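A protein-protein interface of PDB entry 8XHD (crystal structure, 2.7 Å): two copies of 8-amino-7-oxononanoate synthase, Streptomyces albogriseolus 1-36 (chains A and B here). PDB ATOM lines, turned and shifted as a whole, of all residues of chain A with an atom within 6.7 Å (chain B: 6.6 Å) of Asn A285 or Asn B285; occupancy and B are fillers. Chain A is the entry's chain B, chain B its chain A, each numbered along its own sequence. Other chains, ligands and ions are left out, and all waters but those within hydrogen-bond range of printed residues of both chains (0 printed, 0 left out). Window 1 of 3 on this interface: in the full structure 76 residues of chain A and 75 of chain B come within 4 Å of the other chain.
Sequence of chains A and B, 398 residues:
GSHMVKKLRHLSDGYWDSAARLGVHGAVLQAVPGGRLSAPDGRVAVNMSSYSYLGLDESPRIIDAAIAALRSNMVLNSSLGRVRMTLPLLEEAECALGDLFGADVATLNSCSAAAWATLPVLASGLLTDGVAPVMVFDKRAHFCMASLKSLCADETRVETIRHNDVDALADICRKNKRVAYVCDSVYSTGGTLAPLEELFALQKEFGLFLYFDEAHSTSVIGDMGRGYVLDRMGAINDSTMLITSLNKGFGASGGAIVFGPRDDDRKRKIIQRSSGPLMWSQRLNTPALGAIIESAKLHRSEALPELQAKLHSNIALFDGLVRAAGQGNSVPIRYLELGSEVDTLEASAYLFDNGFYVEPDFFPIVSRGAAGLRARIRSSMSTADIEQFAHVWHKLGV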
ATOM      1  N   VAL A  75     -14.452 -25.700  35.408  1.00  0.00           N
ATOM      2  CA  VAL A  75     -14.165 -24.459  36.117  1.00  0.00           C
ATOM      3  C   VAL A  75     -14.262 -23.312  35.122  1.00  0.00           C
ATOM      4  O   VAL A  75     -13.935 -23.461  33.941  1.00  0.00           O
ATOM      5  CB  VAL A  75     -12.775 -24.459  36.796  1.00  0.00           C
ATOM      6  CG1 VAL A  75     -12.713 -25.493  37.916  1.00  0.00           C
ATOM      7  CG2 VAL A  75     -11.679 -24.696  35.765  1.00  0.00           C
ATOM      8  N   LEU A  76     -14.725 -22.158  35.606  1.00  0.00           N
ATOM      9  CA  LEU A  76     -14.751 -20.976  34.751  1.00  0.00           C
ATOM     10  C   LEU A  76     -13.341 -20.510  34.417  1.00  0.00           C
ATOM     11  O   LEU A  76     -13.070 -20.094  33.285  1.00  0.00           O
ATOM     12  CB  LEU A  76     -15.547 -19.856  35.416  1.00  0.00           C
ATOM     13  CG  LEU A  76     -17.063 -19.914  35.215  1.00  0.00           C
ATOM     14  CD1 LEU A  76     -17.760 -18.961  36.168  1.00  0.00           C
ATOM     15  CD2 LEU A  76     -17.428 -19.587  33.774  1.00  0.00           C
ATOM     16  N   ASN A  77     -12.425 -20.592  35.377  1.00  0.00           N
ATOM     17  CA  ASN A  77     -11.056 -20.157  35.154  1.00  0.00           C
ATOM     18  C   ASN A  77     -10.175 -20.763  36.237  1.00  0.00           C
ATOM     19  O   ASN A  77     -10.663 -21.367  37.194  1.00  0.00           O
ATOM     20  CB  ASN A  77     -10.957 -18.627  35.153  1.00  0.00           C
ATOM     21  CG  ASN A  77      -9.806 -18.117  34.312  1.00  0.00           C
ATOM     22  OD1 ASN A  77      -9.104 -18.891  33.660  1.00  0.00           O
ATOM     23  ND2 ASN A  77      -9.614 -16.802  34.311  1.00  0.00           N
ATOM     24  N   LEU A  89      -5.836 -24.972  28.371  1.00  0.00           N
ATOM     25  CA  LEU A  89      -6.754 -24.335  27.437  1.00  0.00           C
ATOM     26  C   LEU A  89      -6.260 -22.946  27.050  1.00  0.00           C
ATOM     27  O   LEU A  89      -6.395 -22.530  25.894  1.00  0.00           O
ATOM     28  CB  LEU A  89      -8.153 -24.263  28.050  1.00  0.00           C
ATOM     29  CG  LEU A  89      -9.295 -23.930  27.092  1.00  0.00           C
ATOM     30  CD1 LEU A  89      -9.415 -25.012  26.033  1.00  0.00           C
ATOM     31  CD2 LEU A  89     -10.603 -23.763  27.847  1.00  0.00           C
ATOM     32  N   ALA A 252     -15.520 -14.179  19.315  1.00  0.00           N
ATOM     33  CA  ALA A 252     -15.220 -14.739  20.626  1.00  0.00           C
ATOM     34  C   ALA A 252     -15.410 -13.692  21.716  1.00  0.00           C
ATOM     35  O   ALA A 252     -16.393 -12.944  21.698  1.00  0.00           O
ATOM     36  CB  ALA A 252     -13.797 -15.297  20.654  1.00  0.00           C
ATOM     37  N   SER A 253     -14.481 -13.632  22.670  1.00  0.00           N
ATOM     38  CA  SER A 253     -14.545 -12.656  23.747  1.00  0.00           C
ATOM     39  C   SER A 253     -13.133 -12.254  24.145  1.00  0.00           C
ATOM     40  O   SER A 253     -12.178 -13.012  23.955  1.00  0.00           O
ATOM     41  CB  SER A 253     -15.301 -13.201  24.967  1.00  0.00           C
ATOM     42  OG  SER A 253     -16.644 -13.506  24.636  1.00  0.00           O
ATOM     43  N   GLN A 282      -7.642 -10.678  35.628  1.00  0.00           N
ATOM     44  CA  GLN A 282      -8.034 -12.059  35.384  1.00  0.00           C
ATOM     45  C   GLN A 282      -7.964 -12.419  33.903  1.00  0.00           C
ATOM     46  O   GLN A 282      -8.291 -11.619  33.020  1.00  0.00           O
ATOM     47  CB  GLN A 282      -9.450 -12.302  35.908  1.00  0.00           C
ATOM     48  CG  GLN A 282     -10.491 -11.330  35.371  1.00  0.00           C
ATOM     49  CD  GLN A 282     -11.862 -11.554  35.981  1.00  0.00           C
ATOM     50  OE1 GLN A 282     -12.606 -12.438  35.556  1.00  0.00           O
ATOM     51  NE2 GLN A 282     -12.201 -10.751  36.984  1.00  0.00           N
ATOM     52  N   ARG A 283      -7.520 -13.648  33.646  1.00  0.00           N
ATOM     53  CA  ARG A 283      -7.507 -14.208  32.307  1.00  0.00           C
ATOM     54  C   ARG A 283      -8.932 -14.452  31.818  1.00  0.00           C
ATOM     55  O   ARG A 283      -9.897 -14.440  32.586  1.00  0.00           O
ATOM     56  CB  ARG A 283      -6.723 -15.518  32.289  1.00  0.00           C
ATOM     57  CG  ARG A 283      -5.335 -15.410  32.889  1.00  0.00           C
ATOM     58  CD  ARG A 283      -4.989 -16.626  33.739  1.00  0.00           C
ATOM     59  NE  ARG A 283      -6.041 -16.961  34.693  1.00  0.00           N
ATOM     60  CZ  ARG A 283      -6.308 -16.275  35.796  1.00  0.00           C
ATOM     61  NH1 ARG A 283      -5.642 -15.173  36.105  1.00  0.00           N
ATOM     62  NH2 ARG A 283      -7.267 -16.703  36.612  1.00  0.00           N
ATOM     63  N   LEU A 284      -9.050 -14.686  30.514  1.00  0.00           N
ATOM     64  CA  LEU A 284     -10.333 -15.054  29.932  1.00  0.00           C
ATOM     65  C   LEU A 284     -10.815 -16.380  30.503  1.00  0.00           C
ATOM     66  O   LEU A 284     -10.020 -17.289  30.760  1.00  0.00           O
ATOM     67  CB  LEU A 284     -10.208 -15.153  28.414  1.00  0.00           C
ATOM     68  CG  LEU A 284     -10.156 -13.833  27.655  1.00  0.00           C
ATOM     69  CD1 LEU A 284      -9.711 -14.073  26.226  1.00  0.00           C
ATOM     70  CD2 LEU A 284     -11.523 -13.183  27.691  1.00  0.00           C
ATOM     71  N   ASN A 285     -12.128 -16.492  30.698  1.00  0.00           N
ATOM     72  CA  ASN A 285     -12.680 -17.723  31.240  1.00  0.00           C
ATOM     73  C   ASN A 285     -12.650 -18.825  30.181  1.00  0.00           C
ATOM     74  O   ASN A 285     -12.401 -18.585  28.997  1.00  0.00           O
ATOM     75  CB  ASN A 285     -14.100 -17.499  31.777  1.00  0.00           C
ATOM     76  CG  ASN A 285     -15.069 -16.967  30.728  1.00  0.00           C
ATOM     77  OD1 ASN A 285     -14.868 -17.122  29.524  1.00  0.00           O
ATOM     78  ND2 ASN A 285     -16.142 -16.340  31.196  1.00  0.00           N
ATOM     79  N   THR A 286     -12.896 -20.056  30.630  1.00  0.00           N
ATOM     80  CA  THR A 286     -12.782 -21.197  29.728  1.00  0.00           C
ATOM     81  C   THR A 286     -13.745 -21.160  28.539  1.00  0.00           C
ATOM     82  O   THR A 286     -13.336 -21.613  27.454  1.00  0.00           O
ATOM     83  CB  THR A 286     -12.941 -22.503  30.526  1.00  0.00           C
ATOM     84  OG1 THR A 286     -14.010 -22.377  31.470  1.00  0.00           O
ATOM     85  CG2 THR A 286     -11.655 -22.825  31.272  1.00  0.00           C
ATOM     86  N   PRO A 287     -14.987 -20.666  28.643  1.00  0.00           N
ATOM     87  CA  PRO A 287     -15.804 -20.555  27.419  1.00  0.00           C
ATOM     88  C   PRO A 287     -15.183 -19.650  26.370  1.00  0.00           C
ATOM     89  O   PRO A 287     -15.133 -20.015  25.188  1.00  0.00           O
ATOM     90  CB  PRO A 287     -17.140 -20.004  27.938  1.00  0.00           C
ATOM     91  CG  PRO A 287     -17.191 -20.421  29.359  1.00  0.00           C
ATOM     92  CD  PRO A 287     -15.778 -20.356  29.848  1.00  0.00           C
ATOM     93  N   ALA A 288     -14.706 -18.470  26.775  1.00  0.00           N
ATOM     94  CA  ALA A 288     -14.075 -17.564  25.822  1.00  0.00           C
ATOM     95  C   ALA A 288     -12.867 -18.212  25.162  1.00  0.00           C
ATOM     96  O   ALA A 288     -12.684 -18.101  23.945  1.00  0.00           O
ATOM     97  CB  ALA A 288     -13.675 -16.264  26.519  1.00  0.00           C
ATOM     98  N   LEU A 289     -12.041 -18.909  25.946  1.00  0.00           N
ATOM     99  CA  LEU A 289     -10.841 -19.524  25.390  1.00  0.00           C
ATOM    100  C   LEU A 289     -11.194 -20.626  24.396  1.00  0.00           C
ATOM    101  O   LEU A 289     -10.551 -20.750  23.349  1.00  0.00           O
ATOM    102  CB  LEU A 289      -9.961 -20.062  26.515  1.00  0.00           C
ATOM    103  CG  LEU A 289      -9.295 -19.009  27.402  1.00  0.00           C
ATOM    104  CD1 LEU A 289      -8.620 -19.659  28.599  1.00  0.00           C
ATOM    105  CD2 LEU A 289      -8.295 -18.187  26.593  1.00  0.00           C
ATOM    106  N   GLY A 290     -12.211 -21.432  24.705  1.00  0.00           N
ATOM    107  CA  GLY A 290     -12.656 -22.432  23.748  1.00  0.00           C
ATOM    108  C   GLY A 290     -13.196 -21.811  22.476  1.00  0.00           C
ATOM    109  O   GLY A 290     -12.994 -22.340  21.379  1.00  0.00           O
ATOM    110  N   VAL B  75     -25.485 -16.971  22.201  1.00  0.00           N
ATOM    111  CA  VAL B  75     -24.540 -15.922  21.842  1.00  0.00           C
ATOM    112  C   VAL B  75     -23.619 -15.702  23.032  1.00  0.00           C
ATOM    113  O   VAL B  75     -24.014 -15.892  24.185  1.00  0.00           O
ATOM    114  CB  VAL B  75     -25.260 -14.615  21.425  1.00  0.00           C
ATOM    115  CG1 VAL B  75     -25.874 -13.925  22.630  1.00  0.00           C
ATOM    116  CG2 VAL B  75     -24.302 -13.683  20.702  1.00  0.00           C
ATOM    117  N   LEU B  76     -22.372 -15.321  22.744  1.00  0.00           N
ATOM    118  CA  LEU B  76     -21.402 -15.122  23.816  1.00  0.00           C
ATOM    119  C   LEU B  76     -21.626 -13.803  24.544  1.00  0.00           C
ATOM    120  O   LEU B  76     -21.655 -13.773  25.779  1.00  0.00           O
ATOM    121  CB  LEU B  76     -19.979 -15.203  23.261  1.00  0.00           C
ATOM    122  CG  LEU B  76     -19.371 -16.606  23.282  1.00  0.00           C
ATOM    123  CD1 LEU B  76     -18.020 -16.630  22.592  1.00  0.00           C
ATOM    124  CD2 LEU B  76     -19.242 -17.093  24.715  1.00  0.00           C
ATOM    125  N   ASN B  77     -21.807 -12.714  23.804  1.00  0.00           N
ATOM    126  CA  ASN B  77     -22.044 -11.400  24.394  1.00  0.00           C
ATOM    127  C   ASN B  77     -23.073 -10.676  23.533  1.00  0.00           C
ATOM    128  O   ASN B  77     -23.862 -11.296  22.811  1.00  0.00           O
ATOM    129  CB  ASN B  77     -20.728 -10.617  24.513  1.00  0.00           C
ATOM    130  CG  ASN B  77     -20.072 -10.391  23.165  1.00  0.00           C
ATOM    131  OD1 ASN B  77     -20.412 -11.050  22.179  1.00  0.00           O
ATOM    132  ND2 ASN B  77     -19.131  -9.458  23.111  1.00  0.00           N
ATOM    133  N   SER B  78     -23.065  -9.349  23.606  1.00  0.00           N
ATOM    134  CA  SER B  78     -23.848  -8.508  22.714  1.00  0.00           C
ATOM    135  C   SER B  78     -22.967  -8.007  21.574  1.00  0.00           C
ATOM    136  O   SER B  78     -21.739  -7.971  21.682  1.00  0.00           O
ATOM    137  CB  SER B  78     -24.455  -7.326  23.473  1.00  0.00           C
ATOM    138  OG  SER B  78     -23.442  -6.475  23.984  1.00  0.00           O
ATOM    139  N   LEU B  89     -30.297 -11.013  30.080  1.00  0.00           N
ATOM    140  CA  LEU B  89     -29.503 -11.722  31.080  1.00  0.00           C
ATOM    141  C   LEU B  89     -28.632 -10.760  31.879  1.00  0.00           C
ATOM    142  O   LEU B  89     -28.400 -10.971  33.074  1.00  0.00           O
ATOM    143  CB  LEU B  89     -28.637 -12.788  30.405  1.00  0.00           C
ATOM    144  CG  LEU B  89     -27.969 -13.796  31.337  1.00  0.00           C
ATOM    145  CD1 LEU B  89     -29.005 -14.719  31.955  1.00  0.00           C
ATOM    146  CD2 LEU B  89     -26.901 -14.604  30.615  1.00  0.00           C
ATOM    147  N   ASN B 109     -15.735  -6.225  32.886  1.00  0.00           N
ATOM    148  CA  ASN B 109     -14.848  -7.340  32.562  1.00  0.00           C
ATOM    149  C   ASN B 109     -13.957  -7.714  33.742  1.00  0.00           C
ATOM    150  O   ASN B 109     -13.579  -8.882  33.886  1.00  0.00           O
ATOM    151  CB  ASN B 109     -13.970  -6.998  31.350  1.00  0.00           C
ATOM    152  CG  ASN B 109     -14.751  -6.416  30.188  1.00  0.00           C
ATOM    153  OD1 ASN B 109     -14.437  -5.328  29.704  1.00  0.00           O
ATOM    154  ND2 ASN B 109     -15.764  -7.142  29.724  1.00  0.00           N
ATOM    155  N   SER B 253     -17.146 -14.683  37.024  1.00  0.00           N
ATOM    156  CA  SER B 253     -16.154 -13.985  36.221  1.00  0.00           C
ATOM    157  C   SER B 253     -16.440 -12.493  36.260  1.00  0.00           C
ATOM    158  O   SER B 253     -17.579 -12.072  36.476  1.00  0.00           O
ATOM    159  CB  SER B 253     -16.153 -14.477  34.769  1.00  0.00           C
ATOM    160  OG  SER B 253     -15.792 -15.846  34.694  1.00  0.00           O
ATOM    161  N   ARG B 283     -18.773  -6.105  27.441  1.00  0.00           N
ATOM    162  CA  ARG B 283     -19.490  -6.596  28.607  1.00  0.00           C
ATOM    163  C   ARG B 283     -19.116  -8.045  28.886  1.00  0.00           C
ATOM    164  O   ARG B 283     -18.573  -8.748  28.029  1.00  0.00           O
ATOM    165  CB  ARG B 283     -20.999  -6.486  28.401  1.00  0.00           C
ATOM    166  CG  ARG B 283     -21.498  -5.086  28.097  1.00  0.00           C
ATOM    167  CD  ARG B 283     -21.658  -4.250  29.358  1.00  0.00           C
ATOM    168  NE  ARG B 283     -20.412  -3.644  29.812  1.00  0.00           N
ATOM    169  CZ  ARG B 283     -19.724  -4.044  30.873  1.00  0.00           C
ATOM    170  NH1 ARG B 283     -20.140  -5.048  31.627  1.00  0.00           N
ATOM    171  NH2 ARG B 283     -18.593  -3.419  31.186  1.00  0.00           N
ATOM    172  N   LEU B 284     -19.418  -8.488  30.107  1.00  0.00           N
ATOM    173  CA  LEU B 284     -19.223  -9.887  30.465  1.00  0.00           C
ATOM    174  C   LEU B 284     -20.022 -10.787  29.530  1.00  0.00           C
ATOM    175  O   LEU B 284     -21.107 -10.426  29.068  1.00  0.00           O
ATOM    176  CB  LEU B 284     -19.640 -10.120  31.919  1.00  0.00           C
ATOM    177  CG  LEU B 284     -18.679  -9.597  32.983  1.00  0.00           C
ATOM    178  CD1 LEU B 284     -19.252  -9.776  34.382  1.00  0.00           C
ATOM    179  CD2 LEU B 284     -17.342 -10.308  32.849  1.00  0.00           C
ATOM    180  N   ASN B 285     -19.473 -11.966  29.242  1.00  0.00           N
ATOM    181  CA  ASN B 285     -20.124 -12.855  28.296  1.00  0.00           C
ATOM    182  C   ASN B 285     -21.290 -13.589  28.955  1.00  0.00           C
ATOM    183  O   ASN B 285     -21.454 -13.592  30.180  1.00  0.00           O
ATOM    184  CB  ASN B 285     -19.123 -13.841  27.683  1.00  0.00           C
ATOM    185  CG  ASN B 285     -18.415 -14.711  28.715  1.00  0.00           C
ATOM    186  OD1 ASN B 285     -18.896 -14.918  29.826  1.00  0.00           O
ATOM    187  ND2 ASN B 285     -17.256 -15.237  28.332  1.00  0.00           N
ATOM    188  N   THR B 286     -22.118 -14.202  28.112  1.00  0.00           N
ATOM    189  CA  THR B 286     -23.279 -14.941  28.588  1.00  0.00           C
ATOM    190  C   THR B 286     -22.946 -16.022  29.625  1.00  0.00           C
ATOM    191  O   THR B 286     -23.703 -16.168  30.581  1.00  0.00           O
ATOM    192  CB  THR B 286     -24.020 -15.548  27.387  1.00  0.00           C
ATOM    193  OG1 THR B 286     -24.257 -14.526  26.413  1.00  0.00           O
ATOM    194  CG2 THR B 286     -25.344 -16.142  27.805  1.00  0.00           C
ATOM    195  N   PRO B 287     -21.852 -16.788  29.478  1.00  0.00           N
ATOM    196  CA  PRO B 287     -21.520 -17.743  30.555  1.00  0.00           C
ATOM    197  C   PRO B 287     -21.260 -17.073  31.888  1.00  0.00           C
ATOM    198  O   PRO B 287     -21.723 -17.560  32.926  1.00  0.00           O
ATOM    199  CB  PRO B 287     -20.260 -18.435  30.015  1.00  0.00           C
ATOM    200  CG  PRO B 287     -20.364 -18.316  28.546  1.00  0.00           C
ATOM    201  CD  PRO B 287     -21.024 -17.002  28.285  1.00  0.00           C
ATOM    202  N   ALA B 288     -20.524 -15.961  31.887  1.00  0.00           N
ATOM    203  CA  ALA B 288     -20.201 -15.277  33.133  1.00  0.00           C
ATOM    204  C   ALA B 288     -21.458 -14.752  33.809  1.00  0.00           C
ATOM    205  O   ALA B 288     -21.645 -14.931  35.018  1.00  0.00           O
ATOM    206  CB  ALA B 288     -19.220 -14.134  32.864  1.00  0.00           C
ATOM    207  N   LEU B 289     -22.333 -14.100  33.038  1.00  0.00           N
ATOM    208  CA  LEU B 289     -23.547 -13.530  33.609  1.00  0.00           C
ATOM    209  C   LEU B 289     -24.432 -14.613  34.208  1.00  0.00           C
ATOM    210  O   LEU B 289     -25.007 -14.427  35.287  1.00  0.00           O
ATOM    211  CB  LEU B 289     -24.302 -12.740  32.542  1.00  0.00           C
ATOM    212  CG  LEU B 289     -23.583 -11.504  32.003  1.00  0.00           C
ATOM    213  CD1 LEU B 289     -24.236 -11.013  30.723  1.00  0.00           C
ATOM    214  CD2 LEU B 289     -23.567 -10.402  33.053  1.00  0.00           C
ATOM    215  N   GLY B 290     -24.552 -15.753  33.523  1.00  0.00           N
ATOM    216  CA  GLY B 290     -25.310 -16.859  34.081  1.00  0.00           C
ATOM    217  C   GLY B 290     -24.724 -17.357  35.388  1.00  0.00           C
ATOM    218  O   GLY B 290     -25.457 -17.761  36.294  1.00  0.00           O
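Of chain B, only Ser B253 and Asn B285 come within 4 Å of Asn A285. Of chain A, only Ser A253 and Asn A285 come within 4 Å of Asn B285. Of the printed residues of chain A, Leu B76 touches Ala A252 (3.9 Å) and Ser A253 (3.98 Å). Printed residues of chain B within 4 Å of Gln A282: Asn B109 (3.8 Å) and Ser B253 (3.9 Å). Of the printed residues of chain A, Pro B287 touches Pro A287 (3.7 Å). Of the printed residues of chain B, Leu A76 touches Ser B253 (3.97 Å). Leu B289 touches none of the printed residues of chain A. The nearest residue of chain B that does not touch Asn A285 is Ala B288 (4.1 Å). The nearest residue of chain A that does not touch Asn B285 is Ala A288 (4.1 Å).
The side-chain amide nitrogen (ND2) of Asn B285 sits close to the side-chain amide nitrogen (ND2) of Asn A285, 3.3 Å away.
Of the 15 printed residues of chain B, 5 touch a printed residue of chain A. Printed residues of chain B that touch a printed residue of chain A: Leu B76, Asn B109, Ser B253, Asn B285 and Pro B287. Hydrophobic or aromatic side chains of chain B that line the printed part of chain A: Leu B76 and Pro B287. Of the 15 printed residues of chain A, 6 touch a printed residue of chain B. Hydrophobic or aromatic side chains of chain A within 4 Å of the printed part of chain B: Leu A76 and Pro A287. Among the printed residues, 9 pairs touch across the chains.
O of Leu B76 is in hydrogen-bond range of N of Thr B286 (2.4 Å). The side-chain amide oxygen (OD1) of Asn B285 lies within hydrogen-bond range of the backbone NH (N) of Ala B288, at 2.8 Å. The backbone carbonyl oxygen (O) of Leu A76 sits at hydrogen-bond distance from the backbone NH (N) of Thr A286. N of Ala A288 sits at hydrogen-bond distance from OD1 of Asn A285, at 3.1 Å.
Leu A76 touches Ser B253. CA of Ala A252 touches CD1 of Leu B76 (3.9 Å). CD1 of Leu B76 touches OG of Ser A253, 3.98 Å away. Asn B285 touches Ser A253. Gln A282 touches Asn B109. OE1 of Gln A282 touches C of Ser B253 (3.9 Å). Asn A285 touches Ser B253. Pro B287 touches Pro A287.
Leu A76 touches Ser B253, and with the chains exchanged Ser A253 touches Leu B76. Ser A253 touches Asn B285, and with the chains exchanged Asn A285 touches Ser B253. Asn B285 touches its own counterpart, Asn A285. Pro B287 touches its own counterpart, Pro A287. Positions printed for both chains: 75, 76, 77, 89, 253, 283, 284, 285, 286, 287, 288, 289 and 290.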
